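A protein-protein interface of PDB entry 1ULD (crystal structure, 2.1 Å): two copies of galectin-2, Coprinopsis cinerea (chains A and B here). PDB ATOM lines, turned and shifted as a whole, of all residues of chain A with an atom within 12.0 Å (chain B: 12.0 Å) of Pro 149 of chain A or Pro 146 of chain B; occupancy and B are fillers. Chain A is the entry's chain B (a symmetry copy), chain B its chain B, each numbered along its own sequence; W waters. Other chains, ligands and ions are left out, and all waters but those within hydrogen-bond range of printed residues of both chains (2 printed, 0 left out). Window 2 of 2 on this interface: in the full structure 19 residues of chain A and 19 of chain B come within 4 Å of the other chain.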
ATOM      1  N   PRO A 145       4.954 -23.853 -10.355  1.00  0.00           N
ATOM      2  CA  PRO A 145       6.167 -24.459 -10.917  1.00  0.00           C
ATOM      3  C   PRO A 145       7.450 -23.737 -10.502  1.00  0.00           C
ATOM      4  O   PRO A 145       7.406 -22.606 -10.013  1.00  0.00           O
ATOM      5  CB  PRO A 145       5.928 -24.350 -12.417  1.00  0.00           C
ATOM      6  CG  PRO A 145       5.236 -23.005 -12.522  1.00  0.00           C
ATOM      7  CD  PRO A 145       4.233 -23.071 -11.377  1.00  0.00           C
ATOM      8  N   PRO A 146       8.611 -24.397 -10.676  1.00  0.00           N
ATOM      9  CA  PRO A 146       9.882 -23.767 -10.315  1.00  0.00           C
ATOM     10  C   PRO A 146       9.943 -22.469 -11.105  1.00  0.00           C
ATOM     11  O   PRO A 146       9.476 -22.410 -12.248  1.00  0.00           O
ATOM     12  CB  PRO A 146      10.912 -24.791 -10.778  1.00  0.00           C
ATOM     13  CG  PRO A 146      10.198 -26.095 -10.522  1.00  0.00           C
ATOM     14  CD  PRO A 146       8.819 -25.800 -11.082  1.00  0.00           C
ATOM     15  N   LEU A 147      10.513 -21.430 -10.509  1.00  0.00           N
ATOM     16  CA  LEU A 147      10.563 -20.132 -11.167  1.00  0.00           C
ATOM     17  C   LEU A 147      11.900 -19.726 -11.767  1.00  0.00           C
ATOM     18  O   LEU A 147      12.961 -20.001 -11.208  1.00  0.00           O
ATOM     19  CB  LEU A 147      10.140 -19.040 -10.177  1.00  0.00           C
ATOM     20  CG  LEU A 147       8.874 -19.274  -9.344  1.00  0.00           C
ATOM     21  CD1 LEU A 147       8.780 -18.217  -8.253  1.00  0.00           C
ATOM     22  CD2 LEU A 147       7.649 -19.240 -10.250  1.00  0.00           C
ATOM     23  N   PRO A 148      11.859 -19.061 -12.927  1.00  0.00           N
ATOM     24  CA  PRO A 148      13.099 -18.613 -13.565  1.00  0.00           C
ATOM     25  C   PRO A 148      13.600 -17.456 -12.701  1.00  0.00           C
ATOM     26  O   PRO A 148      12.809 -16.809 -12.006  1.00  0.00           O
ATOM     27  CB  PRO A 148      12.628 -18.141 -14.941  1.00  0.00           C
ATOM     28  CG  PRO A 148      11.238 -17.640 -14.657  1.00  0.00           C
ATOM     29  CD  PRO A 148      10.691 -18.742 -13.765  1.00  0.00           C
ATOM     30  N   PRO A 149      14.912 -17.182 -12.727  1.00  0.00           N
ATOM     31  CA  PRO A 149      15.467 -16.088 -11.924  1.00  0.00           C
ATOM     32  C   PRO A 149      14.877 -14.734 -12.291  1.00  0.00           C
ATOM     33  O   PRO A 149      15.077 -13.748 -11.586  1.00  0.00           O
ATOM     34  CB  PRO A 149      16.965 -16.171 -12.213  1.00  0.00           C
ATOM     35  CG  PRO A 149      17.006 -16.719 -13.606  1.00  0.00           C
ATOM     36  CD  PRO A 149      15.953 -17.802 -13.563  1.00  0.00           C
ATOM     37  N   ALA A 150      14.148 -14.697 -13.400  1.00  0.00           N
ATOM     38  CA  ALA A 150      13.520 -13.467 -13.867  1.00  0.00           C
ATOM     39  C   ALA A 150      12.667 -13.745 -15.112  1.00  0.00           C
ATOM     40  O   ALA A 150      11.439 -13.505 -15.050  1.00  0.00           O
ATOM     41  CB  ALA A 150      14.593 -12.412 -14.178  1.00  0.00           C
ATOM     42  OXT ALA A 150      13.237 -14.200 -16.129  1.00  0.00           O
ATOM     43  N   MET B   1       6.636 -12.981 -27.144  1.00  0.00           N
ATOM     44  CA  MET B   1       5.448 -12.595 -27.946  1.00  0.00           C
ATOM     45  C   MET B   1       4.614 -13.837 -28.238  1.00  0.00           C
ATOM     46  O   MET B   1       5.112 -14.808 -28.810  1.00  0.00           O
ATOM     47  CB  MET B   1       5.889 -11.954 -29.256  1.00  0.00           C
ATOM     48  CG  MET B   1       4.746 -11.538 -30.153  1.00  0.00           C
ATOM     49  SD  MET B   1       3.799 -10.179 -29.463  1.00  0.00           S
ATOM     50  CE  MET B   1       4.873  -8.813 -29.857  1.00  0.00           C
ATOM     51  N   GLU B  20      19.397 -16.048 -32.487  1.00  0.00           N
ATOM     52  CA  GLU B  20      19.059 -15.916 -31.068  1.00  0.00           C
ATOM     53  C   GLU B  20      17.559 -16.088 -30.832  1.00  0.00           C
ATOM     54  O   GLU B  20      17.129 -16.272 -29.693  1.00  0.00           O
ATOM     55  CB  GLU B  20      19.504 -14.558 -30.505  1.00  0.00           C
ATOM     56  CG  GLU B  20      20.995 -14.246 -30.637  1.00  0.00           C
ATOM     57  CD  GLU B  20      21.883 -15.329 -30.045  1.00  0.00           C
ATOM     58  OE1 GLU B  20      21.592 -15.812 -28.931  1.00  0.00           O
ATOM     59  OE2 GLU B  20      22.887 -15.690 -30.689  1.00  0.00           O
ATOM     60  N   VAL B  22      13.844 -17.719 -30.629  1.00  0.00           N
ATOM     61  CA  VAL B  22      13.329 -19.009 -30.194  1.00  0.00           C
ATOM     62  C   VAL B  22      11.822 -19.048 -30.395  1.00  0.00           C
ATOM     63  O   VAL B  22      11.101 -18.124 -29.997  1.00  0.00           O
ATOM     64  CB  VAL B  22      13.625 -19.257 -28.686  1.00  0.00           C
ATOM     65  CG1 VAL B  22      13.049 -20.611 -28.246  1.00  0.00           C
ATOM     66  CG2 VAL B  22      15.122 -19.197 -28.428  1.00  0.00           C
ATOM     67  N   ALA B  24       8.650 -21.321 -29.445  1.00  0.00           N
ATOM     68  CA  ALA B  24       8.155 -22.438 -28.644  1.00  0.00           C
ATOM     69  C   ALA B  24       6.727 -22.722 -29.074  1.00  0.00           C
ATOM     70  O   ALA B  24       5.809 -21.985 -28.714  1.00  0.00           O
ATOM     71  CB  ALA B  24       8.193 -22.088 -27.159  1.00  0.00           C
ATOM     72  N   ILE B  94      15.002 -22.987 -32.761  1.00  0.00           N
ATOM     73  CA  ILE B  94      15.921 -21.934 -32.390  1.00  0.00           C
ATOM     74  C   ILE B  94      16.842 -21.554 -33.543  1.00  0.00           C
ATOM     75  O   ILE B  94      17.414 -22.423 -34.219  1.00  0.00           O
ATOM     76  CB  ILE B  94      16.765 -22.361 -31.177  1.00  0.00           C
ATOM     77  CG1 ILE B  94      15.833 -22.713 -30.011  1.00  0.00           C
ATOM     78  CG2 ILE B  94      17.727 -21.236 -30.784  1.00  0.00           C
ATOM     79  CD1 ILE B  94      16.554 -23.209 -28.768  1.00  0.00           C
ATOM     80  N   ASP B 139       5.051 -19.131 -28.675  1.00  0.00           N
ATOM     81  CA  ASP B 139       5.736 -18.075 -27.955  1.00  0.00           C
ATOM     82  C   ASP B 139       7.080 -17.856 -28.633  1.00  0.00           C
ATOM     83  O   ASP B 139       7.912 -18.762 -28.683  1.00  0.00           O
ATOM     84  CB  ASP B 139       5.934 -18.458 -26.488  1.00  0.00           C
ATOM     85  CG  ASP B 139       4.671 -18.277 -25.670  1.00  0.00           C
ATOM     86  OD1 ASP B 139       4.247 -17.113 -25.508  1.00  0.00           O
ATOM     87  OD2 ASP B 139       4.105 -19.289 -25.202  1.00  0.00           O
ATOM     88  N   VAL B 140       7.276 -16.648 -29.156  1.00  0.00           N
ATOM     89  CA  VAL B 140       8.500 -16.293 -29.862  1.00  0.00           C
ATOM     90  C   VAL B 140       9.340 -15.308 -29.063  1.00  0.00           C
ATOM     91  O   VAL B 140       8.865 -14.239 -28.666  1.00  0.00           O
ATOM     92  CB  VAL B 140       8.166 -15.687 -31.245  1.00  0.00           C
ATOM     93  CG1 VAL B 140       9.436 -15.438 -32.035  1.00  0.00           C
ATOM     94  CG2 VAL B 140       7.233 -16.631 -32.002  1.00  0.00           C
ATOM     95  N   HIS B 141      10.593 -15.680 -28.838  1.00  0.00           N
ATOM     96  CA  HIS B 141      11.526 -14.870 -28.066  1.00  0.00           C
ATOM     97  C   HIS B 141      12.630 -14.311 -28.954  1.00  0.00           C
ATOM     98  O   HIS B 141      13.044 -14.958 -29.924  1.00  0.00           O
ATOM     99  CB  HIS B 141      12.163 -15.731 -26.974  1.00  0.00           C
ATOM    100  CG  HIS B 141      11.174 -16.508 -26.158  1.00  0.00           C
ATOM    101  ND1 HIS B 141      10.765 -16.111 -24.902  1.00  0.00           N
ATOM    102  CD2 HIS B 141      10.506 -17.657 -26.426  1.00  0.00           C
ATOM    103  CE1 HIS B 141       9.888 -16.981 -24.431  1.00  0.00           C
ATOM    104  NE2 HIS B 141       9.712 -17.929 -25.335  1.00  0.00           N
ATOM    105  N   GLY B 142      13.104 -13.115 -28.611  1.00  0.00           N
ATOM    106  CA  GLY B 142      14.179 -12.491 -29.359  1.00  0.00           C
ATOM    107  C   GLY B 142      15.500 -13.092 -28.910  1.00  0.00           C
ATOM    108  O   GLY B 142      16.513 -13.022 -29.613  1.00  0.00           O
ATOM    109  N   LEU B 143      15.484 -13.684 -27.719  1.00  0.00           N
ATOM    110  CA  LEU B 143      16.659 -14.335 -27.155  1.00  0.00           C
ATOM    111  C   LEU B 143      16.180 -15.377 -26.140  1.00  0.00           C
ATOM    112  O   LEU B 143      15.052 -15.296 -25.650  1.00  0.00           O
ATOM    113  CB  LEU B 143      17.571 -13.314 -26.468  1.00  0.00           C
ATOM    114  CG  LEU B 143      17.229 -12.896 -25.034  1.00  0.00           C
ATOM    115  CD1 LEU B 143      18.301 -11.942 -24.518  1.00  0.00           C
ATOM    116  CD2 LEU B 143      15.855 -12.241 -24.985  1.00  0.00           C
ATOM    117  N   LEU B 144      17.020 -16.363 -25.840  1.00  0.00           N
ATOM    118  CA  LEU B 144      16.644 -17.387 -24.868  1.00  0.00           C
ATOM    119  C   LEU B 144      16.375 -16.687 -23.528  1.00  0.00           C
ATOM    120  O   LEU B 144      17.227 -15.967 -23.018  1.00  0.00           O
ATOM    121  CB  LEU B 144      17.772 -18.407 -24.704  1.00  0.00           C
ATOM    122  CG  LEU B 144      17.421 -19.694 -23.953  1.00  0.00           C
ATOM    123  CD1 LEU B 144      16.500 -20.558 -24.810  1.00  0.00           C
ATOM    124  CD2 LEU B 144      18.705 -20.452 -23.620  1.00  0.00           C
ATOM    125  N   PRO B 145      15.180 -16.890 -22.947  1.00  0.00           N
ATOM    126  CA  PRO B 145      14.832 -16.259 -21.668  1.00  0.00           C
ATOM    127  C   PRO B 145      15.504 -16.925 -20.465  1.00  0.00           C
ATOM    128  O   PRO B 145      16.014 -18.043 -20.567  1.00  0.00           O
ATOM    129  CB  PRO B 145      13.319 -16.419 -21.619  1.00  0.00           C
ATOM    130  CG  PRO B 145      13.134 -17.789 -22.242  1.00  0.00           C
ATOM    131  CD  PRO B 145      14.069 -17.726 -23.443  1.00  0.00           C
ATOM    132  N   PRO B 146      15.526 -16.231 -19.311  1.00  0.00           N
ATOM    133  CA  PRO B 146      16.138 -16.807 -18.113  1.00  0.00           C
ATOM    134  C   PRO B 146      15.418 -18.124 -17.869  1.00  0.00           C
ATOM    135  O   PRO B 146      14.211 -18.231 -18.112  1.00  0.00           O
ATOM    136  CB  PRO B 146      15.841 -15.762 -17.044  1.00  0.00           C
ATOM    137  CG  PRO B 146      15.914 -14.476 -17.829  1.00  0.00           C
ATOM    138  CD  PRO B 146      15.117 -14.833 -19.071  1.00  0.00           C
ATOM    139  N   LEU B 147      16.145 -19.125 -17.391  1.00  0.00           N
ATOM    140  CA  LEU B 147      15.553 -20.439 -17.182  1.00  0.00           C
ATOM    141  C   LEU B 147      15.226 -20.816 -15.745  1.00  0.00           C
ATOM    142  O   LEU B 147      15.962 -20.489 -14.815  1.00  0.00           O
ATOM    143  CB  LEU B 147      16.484 -21.516 -17.752  1.00  0.00           C
ATOM    144  CG  LEU B 147      17.058 -21.302 -19.157  1.00  0.00           C
ATOM    145  CD1 LEU B 147      18.149 -22.331 -19.423  1.00  0.00           C
ATOM    146  CD2 LEU B 147      15.942 -21.404 -20.190  1.00  0.00           C
ATOM    147  N   PRO B 148      14.103 -21.515 -15.550  1.00  0.00           N
ATOM    148  CA  PRO B 148      13.721 -21.938 -14.201  1.00  0.00           C
ATOM    149  C   PRO B 148      14.703 -23.052 -13.837  1.00  0.00           C
ATOM    150  O   PRO B 148      15.259 -23.705 -14.725  1.00  0.00           O
ATOM    151  CB  PRO B 148      12.298 -22.464 -14.393  1.00  0.00           C
ATOM    152  CG  PRO B 148      12.337 -23.004 -15.796  1.00  0.00           C
ATOM    153  CD  PRO B 148      13.073 -21.897 -16.532  1.00  0.00           C
ATOM    154  N   PRO B 149      14.930 -23.281 -12.536  1.00  0.00           N
ATOM    155  CA  PRO B 149      15.860 -24.333 -12.110  1.00  0.00           C
ATOM    156  C   PRO B 149      15.435 -25.716 -12.582  1.00  0.00           C
ATOM    157  O   PRO B 149      16.198 -26.674 -12.490  1.00  0.00           O
ATOM    158  CB  PRO B 149      15.852 -24.207 -10.587  1.00  0.00           C
ATOM    159  CG  PRO B 149      14.472 -23.697 -10.302  1.00  0.00           C
ATOM    160  CD  PRO B 149      14.282 -22.650 -11.376  1.00  0.00           C
ATOM    161  N   ALA B 150      14.213 -25.809 -13.091  1.00  0.00           N
ATOM    162  CA  ALA B 150      13.679 -27.072 -13.585  1.00  0.00           C
ATOM    163  C   ALA B 150      12.289 -26.860 -14.198  1.00  0.00           C
ATOM    164  O   ALA B 150      12.129 -27.139 -15.409  1.00  0.00           O
ATOM    165  CB  ALA B 150      13.609 -28.098 -12.443  1.00  0.00           C
ATOM    166  OXT ALA B 150      11.380 -26.415 -13.461  1.00  0.00           O
HETATM  167  O   HOH W   1       9.447 -24.416 -14.222  1.00  0.00           O
HETATM  168  O   HOH W   2      12.199 -16.284 -17.828  1.00  0.00           O
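Pro 148 of chain B touches Pro 146 of chain A.
CB of Pro 146 of chain A touches CG of Pro 149 of chain B, at 3.8 Å.
OXT of Ala 150 of chain B touches CB of Pro 146 of chain A, at 3.2 Å.
O of Leu 147 of chain A touches CA of Pro 148 of chain B (3.6 Å).
Leu 147 of chain A touches Pro 149 of chain B (O to CD, 3.0 Å).
Pro 148 of chain A touches Pro 146 of chain B (CB to O, 3.5 Å).
CA of Pro 148 of chain A touches O of Leu 147 of chain B (3.6 Å).
CG of Pro 149 of chain A touches CB of Pro 146 of chain B, at 3.8 Å.
CD of Pro 149 of chain A touches O of Leu 147 of chain B, 3.0 Å away.
Pro 146 of chain B touches Ala 150 of chain A (CB to OXT, 3.2 Å).
Pro 149 of chain A touches just these residues of chain B: Pro 146 (3.8 Å) and Leu 147 (3.0 Å).
Pro 146 of chain B touches just these residues of chain A: Pro 148, Pro 149 and Ala 150.
Leu 147 of chain A touches two residues of chain B.
Printed residues of chain B within 4 Å of Pro 148 of chain A: Pro 146 (3.5 Å), Leu 147 (3.6 Å) and Pro 148 (3.4 Å).
Ala 150 of chain A touches just one residue of chain B: Pro 146 (3.2 Å).
No residue of chain A comes within 4 Å of Leu 144 of chain B.
No residue of chain A comes within 4 Å of Pro 145 of chain B.
Of chain A, only Pro 148 (3.6 Å) and Pro 149 (3.0 Å) come within 4 Å of Leu 147 of chain B.
Pro 148 of chain B touches just these residues of chain A: Pro 146 (3.5 Å), Leu 147 (3.6 Å) and Pro 148 (3.4 Å).
Of the printed residues of chain A, Pro 149 of chain B touches Pro 146 and Leu 147.
Printed residues of chain A within 4 Å of Ala 150 of chain B: Pro 146.
Of the printed residues of chain B, Pro 146 of chain A touches Pro 148 (3.5 Å), Pro 149 (3.8 Å) and Ala 150 (3.2 Å).
Val 22 of chain B touches none of the printed residues of chain A.
The nearest printed residue of chain A that does not touch Pro 149 of chain B is Pro 148 of chain A (4.6 Å).
Hydrophobic or aromatic side chains of chain B that line the printed part of chain A: Pro 146, Pro 148 and Pro 149.
Of the 6 printed residues of chain A, 5 touch a printed residue of chain B.
Among the printed residues, no Asp or Glu carboxylate lies within 4 Å of a Lys or Arg side-chain nitrogen of the other chain.
Pro 146 of chain A touches Pro 148 of chain B, and with the chains exchanged Pro 148 of chain A touches Pro 146 of chain B.
Pro 146 of chain A touches Pro 149 of chain B, and with the chains exchanged Pro 149 of chain A touches Pro 146 of chain B.
Pro 146 of chain A touches Ala 150 of chain B, and with the chains exchanged Ala 150 of chain A touches Pro 146 of chain B.
Leu 147 of chain A touches Pro 149 of chain B, and with the chains exchanged Pro 149 of chain A touches Leu 147 of chain B.
Of the 11 pairs that touch across the chains among the printed residues, 11 have their exchanged pair printed and touching as well.
Water W1 lies within hydrogen-bond range of O of Pro 146 of chain A and OXT of Ala 150 of chain B.
Water W2 lies within hydrogen-bond range of O of Pro 146 of chain B (2.8 Å) and OXT of Ala 150 of chain A (2.9 Å).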
